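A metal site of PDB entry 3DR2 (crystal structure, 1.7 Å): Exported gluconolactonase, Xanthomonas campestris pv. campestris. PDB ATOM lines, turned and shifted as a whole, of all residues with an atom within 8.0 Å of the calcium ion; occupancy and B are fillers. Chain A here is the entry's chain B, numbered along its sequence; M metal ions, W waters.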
ATOM      1  N   TRP A  46      16.472 -26.074 -25.052  1.00  0.00           N
ATOM      2  CA  TRP A  46      15.020 -25.925 -25.193  1.00  0.00           C
ATOM      3  C   TRP A  46      14.369 -27.266 -25.518  1.00  0.00           C
ATOM      4  O   TRP A  46      14.149 -27.587 -26.694  1.00  0.00           O
ATOM      5  CB  TRP A  46      14.724 -24.901 -26.292  1.00  0.00           C
ATOM      6  CG  TRP A  46      13.288 -24.462 -26.349  1.00  0.00           C
ATOM      7  CD1 TRP A  46      12.226 -25.204 -26.737  1.00  0.00           C
ATOM      8  CD2 TRP A  46      12.774 -23.159 -26.000  1.00  0.00           C
ATOM      9  NE1 TRP A  46      11.069 -24.458 -26.663  1.00  0.00           N
ATOM     10  CE2 TRP A  46      11.375 -23.199 -26.212  1.00  0.00           C
ATOM     11  CE3 TRP A  46      13.357 -21.977 -25.551  1.00  0.00           C
ATOM     12  CZ2 TRP A  46      10.553 -22.094 -25.975  1.00  0.00           C
ATOM     13  CZ3 TRP A  46      12.538 -20.870 -25.300  1.00  0.00           C
ATOM     14  CH2 TRP A  46      11.145 -20.941 -25.516  1.00  0.00           C
ATOM     15  N   SER A  47      14.057 -28.042 -24.486  1.00  0.00           N
ATOM     16  CA  SER A  47      13.465 -29.369 -24.656  1.00  0.00           C
ATOM     17  C   SER A  47      12.028 -29.320 -25.151  1.00  0.00           C
ATOM     18  O   SER A  47      11.221 -28.528 -24.659  1.00  0.00           O
ATOM     19  CB  SER A  47      13.547 -30.153 -23.346  1.00  0.00           C
ATOM     20  OG  SER A  47      14.901 -30.348 -22.966  1.00  0.00           O
ATOM     21  N   GLU A  48      11.724 -30.182 -26.120  1.00  0.00           N
ATOM     22  CA  GLU A  48      10.408 -30.225 -26.743  1.00  0.00           C
ATOM     23  C   GLU A  48      10.020 -31.615 -27.245  1.00  0.00           C
ATOM     24  O   GLU A  48      10.848 -32.518 -27.294  1.00  0.00           O
ATOM     25  CB  GLU A  48      10.391 -29.283 -27.958  1.00  0.00           C
ATOM     26  CG  GLU A  48      10.456 -27.824 -27.634  1.00  0.00           C
ATOM     27  CD  GLU A  48       9.086 -27.240 -27.413  1.00  0.00           C
ATOM     28  OE1 GLU A  48       8.220 -27.975 -26.894  1.00  0.00           O
ATOM     29  OE2 GLU A  48       8.875 -26.059 -27.749  1.00  0.00           O
ATOM     30  N   GLY A  49       8.763 -31.718 -27.637  1.00  0.00           N
ATOM     31  CA  GLY A  49       8.188 -32.924 -28.215  1.00  0.00           C
ATOM     32  C   GLY A  49       8.605 -34.312 -27.773  1.00  0.00           C
ATOM     33  O   GLY A  49       9.187 -35.071 -28.559  1.00  0.00           O
ATOM     34  N   LEU A  64      15.260 -28.272 -29.305  1.00  0.00           N
ATOM     35  CA  LEU A  64      15.000 -27.399 -30.440  1.00  0.00           C
ATOM     36  C   LEU A  64      16.123 -26.406 -30.721  1.00  0.00           C
ATOM     37  O   LEU A  64      16.592 -26.304 -31.860  1.00  0.00           O
ATOM     38  CB  LEU A  64      13.685 -26.654 -30.209  1.00  0.00           C
ATOM     39  CG  LEU A  64      13.264 -25.586 -31.216  1.00  0.00           C
ATOM     40  CD1 LEU A  64      13.137 -26.194 -32.602  1.00  0.00           C
ATOM     41  CD2 LEU A  64      11.931 -24.995 -30.784  1.00  0.00           C
ATOM     42  N   ASN A  89      11.126 -29.841 -33.699  1.00  0.00           N
ATOM     43  CA  ASN A  89      10.340 -29.516 -32.515  1.00  0.00           C
ATOM     44  C   ASN A  89       9.576 -30.773 -32.078  1.00  0.00           C
ATOM     45  O   ASN A  89      10.145 -31.654 -31.414  1.00  0.00           O
ATOM     46  CB  ASN A  89       9.384 -28.360 -32.857  1.00  0.00           C
ATOM     47  CG  ASN A  89       8.669 -27.787 -31.637  1.00  0.00           C
ATOM     48  OD1 ASN A  89       8.104 -26.685 -31.700  1.00  0.00           O
ATOM     49  ND2 ASN A  89       8.682 -28.525 -30.530  1.00  0.00           N
ATOM     50  N   GLY A  90       8.315 -30.889 -32.474  1.00  0.00           N
ATOM     51  CA  GLY A  90       7.544 -32.052 -32.079  1.00  0.00           C
ATOM     52  C   GLY A  90       8.024 -33.373 -32.673  1.00  0.00           C
ATOM     53  O   GLY A  90       8.588 -33.412 -33.767  1.00  0.00           O
ATOM     54  N   HIS A 104      11.039 -26.886 -37.723  1.00  0.00           N
ATOM     55  CA  HIS A 104      10.873 -25.442 -37.918  1.00  0.00           C
ATOM     56  C   HIS A 104      11.692 -24.963 -39.105  1.00  0.00           C
ATOM     57  O   HIS A 104      11.230 -24.148 -39.897  1.00  0.00           O
ATOM     58  CB  HIS A 104      11.345 -24.664 -36.686  1.00  0.00           C
ATOM     59  CG  HIS A 104      10.340 -24.603 -35.579  1.00  0.00           C
ATOM     60  ND1 HIS A 104      10.535 -23.831 -34.457  1.00  0.00           N
ATOM     61  CD2 HIS A 104       9.141 -25.205 -35.406  1.00  0.00           C
ATOM     62  CE1 HIS A 104       9.497 -23.956 -33.644  1.00  0.00           C
ATOM     63  NE2 HIS A 104       8.638 -24.787 -34.206  1.00  0.00           N
ATOM     64  N   PRO A 133       5.647 -26.192 -38.784  1.00  0.00           N
ATOM     65  CA  PRO A 133       5.028 -27.274 -38.015  1.00  0.00           C
ATOM     66  C   PRO A 133       5.563 -27.288 -36.584  1.00  0.00           C
ATOM     67  O   PRO A 133       6.774 -27.261 -36.375  1.00  0.00           O
ATOM     68  CB  PRO A 133       5.385 -28.509 -38.823  1.00  0.00           C
ATOM     69  CG  PRO A 133       5.304 -27.986 -40.226  1.00  0.00           C
ATOM     70  CD  PRO A 133       6.050 -26.666 -40.123  1.00  0.00           C
ATOM     71  N   ASN A 134       4.657 -27.332 -35.619  1.00  0.00           N
ATOM     72  CA  ASN A 134       5.028 -27.271 -34.216  1.00  0.00           C
ATOM     73  C   ASN A 134       4.909 -28.579 -33.451  1.00  0.00           C
ATOM     74  O   ASN A 134       5.861 -29.021 -32.813  1.00  0.00           O
ATOM     75  CB  ASN A 134       4.171 -26.194 -33.538  1.00  0.00           C
ATOM     76  CG  ASN A 134       4.691 -25.819 -32.168  1.00  0.00           C
ATOM     77  OD1 ASN A 134       4.580 -26.592 -31.221  1.00  0.00           O
ATOM     78  ND2 ASN A 134       5.243 -24.614 -32.059  1.00  0.00           N
ATOM     79  N   ASP A 135       3.734 -29.203 -33.490  1.00  0.00           N
ATOM     80  CA  ASP A 135       3.536 -30.462 -32.781  1.00  0.00           C
ATOM     81  C   ASP A 135       2.737 -31.371 -33.701  1.00  0.00           C
ATOM     82  O   ASP A 135       2.023 -30.893 -34.582  1.00  0.00           O
ATOM     83  CB  ASP A 135       2.809 -30.212 -31.453  1.00  0.00           C
ATOM     84  CG  ASP A 135       3.091 -31.268 -30.405  1.00  0.00           C
ATOM     85  OD1 ASP A 135       2.774 -31.027 -29.209  1.00  0.00           O
ATOM     86  OD2 ASP A 135       3.624 -32.340 -30.763  1.00  0.00           O
ATOM     87  N   LEU A 136       2.857 -32.681 -33.502  1.00  0.00           N
ATOM     88  CA  LEU A 136       2.147 -33.633 -34.346  1.00  0.00           C
ATOM     89  C   LEU A 136       1.803 -34.905 -33.605  1.00  0.00           C
ATOM     90  O   LEU A 136       2.373 -35.200 -32.555  1.00  0.00           O
ATOM     91  CB  LEU A 136       2.995 -33.986 -35.582  1.00  0.00           C
ATOM     92  CG  LEU A 136       4.154 -34.986 -35.407  1.00  0.00           C
ATOM     93  CD1 LEU A 136       4.848 -35.175 -36.753  1.00  0.00           C
ATOM     94  CD2 LEU A 136       5.161 -34.471 -34.376  1.00  0.00           C
ATOM     95  N   THR A 147       0.050 -29.163 -36.071  1.00  0.00           N
ATOM     96  CA  THR A 147      -0.270 -27.745 -35.961  1.00  0.00           C
ATOM     97  C   THR A 147       0.756 -26.899 -36.704  1.00  0.00           C
ATOM     98  O   THR A 147       1.936 -27.231 -36.720  1.00  0.00           O
ATOM     99  CB  THR A 147      -0.281 -27.309 -34.492  1.00  0.00           C
ATOM    100  OG1 THR A 147       0.962 -27.669 -33.883  1.00  0.00           O
ATOM    101  CG2 THR A 147      -1.409 -27.994 -33.759  1.00  0.00           C
ATOM    102  N   PRO A 149       1.662 -23.179 -36.377  1.00  0.00           N
ATOM    103  CA  PRO A 149       1.731 -21.779 -35.936  1.00  0.00           C
ATOM    104  C   PRO A 149       3.000 -21.178 -36.561  1.00  0.00           C
ATOM    105  O   PRO A 149       3.848 -21.917 -37.076  1.00  0.00           O
ATOM    106  CB  PRO A 149       1.828 -21.901 -34.435  1.00  0.00           C
ATOM    107  CG  PRO A 149       2.660 -23.137 -34.275  1.00  0.00           C
ATOM    108  CD  PRO A 149       2.055 -24.091 -35.293  1.00  0.00           C
ATOM    109  N   PHE A 151       5.548 -19.753 -35.068  1.00  0.00           N
ATOM    110  CA  PHE A 151       6.638 -19.602 -34.117  1.00  0.00           C
ATOM    111  C   PHE A 151       8.023 -19.787 -34.721  1.00  0.00           C
ATOM    112  O   PHE A 151       8.943 -19.039 -34.400  1.00  0.00           O
ATOM    113  CB  PHE A 151       6.440 -20.548 -32.929  1.00  0.00           C
ATOM    114  CG  PHE A 151       5.272 -20.178 -32.068  1.00  0.00           C
ATOM    115  CD1 PHE A 151       5.205 -18.914 -31.476  1.00  0.00           C
ATOM    116  CD2 PHE A 151       4.230 -21.069 -31.847  1.00  0.00           C
ATOM    117  CE1 PHE A 151       4.118 -18.543 -30.697  1.00  0.00           C
ATOM    118  CE2 PHE A 151       3.135 -20.713 -31.064  1.00  0.00           C
ATOM    119  CZ  PHE A 151       3.081 -19.454 -30.489  1.00  0.00           C
ATOM    120  N   PRO A 190      -2.047 -22.261 -33.191  1.00  0.00           N
ATOM    121  CA  PRO A 190      -2.320 -23.612 -32.708  1.00  0.00           C
ATOM    122  C   PRO A 190      -0.987 -24.191 -32.237  1.00  0.00           C
ATOM    123  O   PRO A 190       0.045 -23.936 -32.850  1.00  0.00           O
ATOM    124  CB  PRO A 190      -2.884 -24.313 -33.940  1.00  0.00           C
ATOM    125  CG  PRO A 190      -2.204 -23.620 -35.064  1.00  0.00           C
ATOM    126  CD  PRO A 190      -2.254 -22.167 -34.643  1.00  0.00           C
ATOM    127  N   ASN A 191      -1.016 -24.962 -31.161  1.00  0.00           N
ATOM    128  CA  ASN A 191       0.227 -25.481 -30.623  1.00  0.00           C
ATOM    129  C   ASN A 191       0.221 -26.995 -30.411  1.00  0.00           C
ATOM    130  O   ASN A 191       0.647 -27.745 -31.284  1.00  0.00           O
ATOM    131  CB  ASN A 191       0.515 -24.775 -29.299  1.00  0.00           C
ATOM    132  CG  ASN A 191       1.984 -24.632 -29.036  1.00  0.00           C
ATOM    133  OD1 ASN A 191       2.757 -25.550 -29.283  1.00  0.00           O
ATOM    134  ND2 ASN A 191       2.395 -23.475 -28.526  1.00  0.00           N
ATOM    135  N   GLY A 192      -0.220 -27.438 -29.249  1.00  0.00           N
ATOM    136  CA  GLY A 192      -0.236 -28.866 -28.990  1.00  0.00           C
ATOM    137  C   GLY A 192      -1.529 -29.492 -29.494  1.00  0.00           C
ATOM    138  O   GLY A 192      -2.487 -28.793 -29.833  1.00  0.00           O
ATOM    139  N   LEU A 193      -1.550 -30.817 -29.577  1.00  0.00           N
ATOM    140  CA  LEU A 193      -2.745 -31.526 -30.009  1.00  0.00           C
ATOM    141  C   LEU A 193      -2.717 -32.967 -29.552  1.00  0.00           C
ATOM    142  O   LEU A 193      -1.657 -33.532 -29.290  1.00  0.00           O
ATOM    143  CB  LEU A 193      -2.904 -31.457 -31.532  1.00  0.00           C
ATOM    144  CG  LEU A 193      -1.977 -32.289 -32.422  1.00  0.00           C
ATOM    145  CD1 LEU A 193      -2.410 -32.103 -33.863  1.00  0.00           C
ATOM    146  CD2 LEU A 193      -0.530 -31.871 -32.239  1.00  0.00           C
ATOM    147  N   SER A 205      -4.363 -26.925 -28.641  1.00  0.00           N
ATOM    148  CA  SER A 205      -4.226 -25.719 -27.842  1.00  0.00           C
ATOM    149  C   SER A 205      -3.915 -24.536 -28.738  1.00  0.00           C
ATOM    150  O   SER A 205      -3.427 -24.702 -29.855  1.00  0.00           O
ATOM    151  CB  SER A 205      -3.125 -25.879 -26.767  1.00  0.00           C
ATOM    152  OG  SER A 205      -1.843 -26.089 -27.318  1.00  0.00           O
ATOM    153  N   THR A 207      -2.086 -20.751 -28.426  1.00  0.00           N
ATOM    154  CA  THR A 207      -1.269 -19.934 -27.540  1.00  0.00           C
ATOM    155  C   THR A 207      -0.776 -18.615 -28.128  1.00  0.00           C
ATOM    156  O   THR A 207       0.422 -18.402 -28.295  1.00  0.00           O
ATOM    157  CB  THR A 207      -0.044 -20.743 -27.064  1.00  0.00           C
ATOM    158  OG1 THR A 207       0.786 -21.078 -28.190  1.00  0.00           O
ATOM    159  CG2 THR A 207      -0.476 -22.039 -26.390  1.00  0.00           C
ATOM    160  N   PRO A 241      -0.757 -23.512 -22.292  1.00  0.00           N
ATOM    161  CA  PRO A 241      -1.007 -24.949 -22.399  1.00  0.00           C
ATOM    162  C   PRO A 241      -0.324 -25.232 -23.737  1.00  0.00           C
ATOM    163  O   PRO A 241      -0.951 -25.176 -24.791  1.00  0.00           O
ATOM    164  CB  PRO A 241      -2.522 -25.028 -22.487  1.00  0.00           C
ATOM    165  CG  PRO A 241      -2.873 -23.780 -23.250  1.00  0.00           C
ATOM    166  CD  PRO A 241      -1.978 -22.739 -22.610  1.00  0.00           C
ATOM    167  N   ASP A 242       0.979 -25.490 -23.679  1.00  0.00           N
ATOM    168  CA  ASP A 242       1.795 -25.724 -24.861  1.00  0.00           C
ATOM    169  C   ASP A 242       1.508 -27.113 -25.435  1.00  0.00           C
ATOM    170  O   ASP A 242       0.635 -27.288 -26.281  1.00  0.00           O
ATOM    171  CB  ASP A 242       3.270 -25.594 -24.481  1.00  0.00           C
ATOM    172  CG  ASP A 242       4.162 -25.268 -25.659  1.00  0.00           C
ATOM    173  OD1 ASP A 242       3.950 -25.825 -26.744  1.00  0.00           O
ATOM    174  OD2 ASP A 242       5.110 -24.458 -25.484  1.00  0.00           O
ATOM    175  N   GLY A 243       2.279 -28.096 -24.972  1.00  0.00           N
ATOM    176  CA  GLY A 243       2.091 -29.465 -25.415  1.00  0.00           C
ATOM    177  C   GLY A 243       1.343 -30.226 -24.333  1.00  0.00           C
ATOM    178  O   GLY A 243       1.414 -29.876 -23.153  1.00  0.00           O
ATOM    179  N   PHE A 244       0.619 -31.261 -24.724  1.00  0.00           N
ATOM    180  CA  PHE A 244      -0.161 -32.044 -23.771  1.00  0.00           C
ATOM    181  C   PHE A 244      -0.457 -33.416 -24.345  1.00  0.00           C
ATOM    182  O   PHE A 244      -0.218 -33.672 -25.530  1.00  0.00           O
ATOM    183  CB  PHE A 244      -1.455 -31.307 -23.449  1.00  0.00           C
ATOM    184  CG  PHE A 244      -2.286 -30.980 -24.663  1.00  0.00           C
ATOM    185  CD1 PHE A 244      -3.119 -31.943 -25.239  1.00  0.00           C
ATOM    186  CD2 PHE A 244      -2.222 -29.723 -25.249  1.00  0.00           C
ATOM    187  CE1 PHE A 244      -3.870 -31.640 -26.378  1.00  0.00           C
ATOM    188  CE2 PHE A 244      -2.966 -29.416 -26.383  1.00  0.00           C
ATOM    189  CZ  PHE A 244      -3.791 -30.376 -26.954  1.00  0.00           C
ATOM    190  N   SER A 255       0.905 -29.307 -20.216  1.00  0.00           N
ATOM    191  CA  SER A 255       2.014 -28.493 -19.739  1.00  0.00           C
ATOM    192  C   SER A 255       1.433 -27.131 -19.357  1.00  0.00           C
ATOM    193  O   SER A 255       0.301 -26.818 -19.726  1.00  0.00           O
ATOM    194  CB  SER A 255       3.053 -28.305 -20.854  1.00  0.00           C
ATOM    195  OG  SER A 255       2.494 -27.630 -21.978  1.00  0.00           O
ATOM    196  N   SER A 280       7.030 -27.478 -21.306  1.00  0.00           N
ATOM    197  CA  SER A 280       6.670 -27.266 -22.701  1.00  0.00           C
ATOM    198  C   SER A 280       5.811 -28.388 -23.293  1.00  0.00           C
ATOM    199  O   SER A 280       5.046 -28.147 -24.208  1.00  0.00           O
ATOM    200  CB  SER A 280       7.929 -27.125 -23.562  1.00  0.00           C
ATOM    201  OG  SER A 280       8.656 -28.342 -23.573  1.00  0.00           O
ATOM    202  N   ASN A 281       5.948 -29.595 -22.769  1.00  0.00           N
ATOM    203  CA  ASN A 281       5.204 -30.715 -23.319  1.00  0.00           C
ATOM    204  C   ASN A 281       5.272 -31.900 -22.362  1.00  0.00           C
ATOM    205  O   ASN A 281       5.974 -31.844 -21.346  1.00  0.00           O
ATOM    206  CB  ASN A 281       5.822 -31.118 -24.661  1.00  0.00           C
ATOM    207  CG  ASN A 281       4.808 -31.602 -25.666  1.00  0.00           C
ATOM    208  OD1 ASN A 281       3.947 -32.412 -25.348  1.00  0.00           O
ATOM    209  ND2 ASN A 281       4.900 -31.108 -26.896  1.00  0.00           N
HETATM  210 CA    CA M   1       4.607 -26.900 -28.796  1.00  0.00          CA
HETATM  211  O   HOH W   1       6.549 -25.433 -29.038  1.00  0.00           O
HETATM  212  O   HOH W   2       5.804 -28.750 -29.969  1.00  0.00           O
HETATM  213  O   HOH W   3       2.943 -28.426 -28.376  1.00  0.00           O
HETATM  214  O   HOH W   4       5.708 -28.034 -26.978  1.00  0.00           O
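The side-chain amide oxygen (OD1) of Asn 89 lies close to the backbone carbonyl oxygen (O) of Asn 134.
The side-chain hydroxyl (OG) of Ser 255 is in hydrogen-bond range of the backbone NH (N) of Asp 242 (3.1 Å).
The backbone carbonyl oxygen of Thr 147 sits at hydrogen-bond distance from the backbone NH of Asn 134 (2.9 Å).
OG1 of Thr 147 is in hydrogen-bond range of O of Asn 191 (2.6 Å).
O of Ser 205 sits at hydrogen-bond distance from N of Asn 191, 2.8 Å away.
The backbone NH (N) of Gly 192 lies within hydrogen-bond range of the backbone carbonyl oxygen (O) of Asp 242, at 3.1 Å.
The side-chain hydroxyl (OG) of Ser 205 sits at hydrogen-bond distance from the backbone carbonyl oxygen (O) of Asp 242 (2.9 Å).
The backbone carbonyl oxygen (O) of Asn 134 sits at hydrogen-bond distance from the backbone NH (N) of Gly 90, at 3.1 Å.
Three residues have an atom within 4 Å of the calcium ion: Asn 134, Asn 191 and Asp 242.
The nearest printed residue that does not touch the calcium ion is Glu 48 (4.2 Å).
The calcium ion is bound by water W3 (2.3 Å), OD1 of Asn 191 (2.3 Å), OD1 of Asp 242 (2.4 Å), water W4 (2.4 Å), OD1 of Asn 134 (2.4 Å), water W1 (2.4 Å) and water W2 (2.5 Å).
The calcium ion has seven donor atoms within binding distance.
Water W2 lies within hydrogen-bond range of the backbone carbonyl oxygen of Asn 134 and the side-chain amide nitrogen of Asn 89.
Water W4 lies within hydrogen-bond range of OE1 of Glu 48, O of Ser 280 and ND2 of Asn 281.
Water W1 lies within hydrogen-bond range of OE2 of Glu 48, OD1 of Asn 89 and ND2 of Asn 134.
Water W3 lies within hydrogen-bond range of OD1 of Asp 135 (2.7 Å), O of Asp 242 (3.3 Å), N of Gly 192 (3.4 Å) and N of Gly 243 (3.5 Å).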
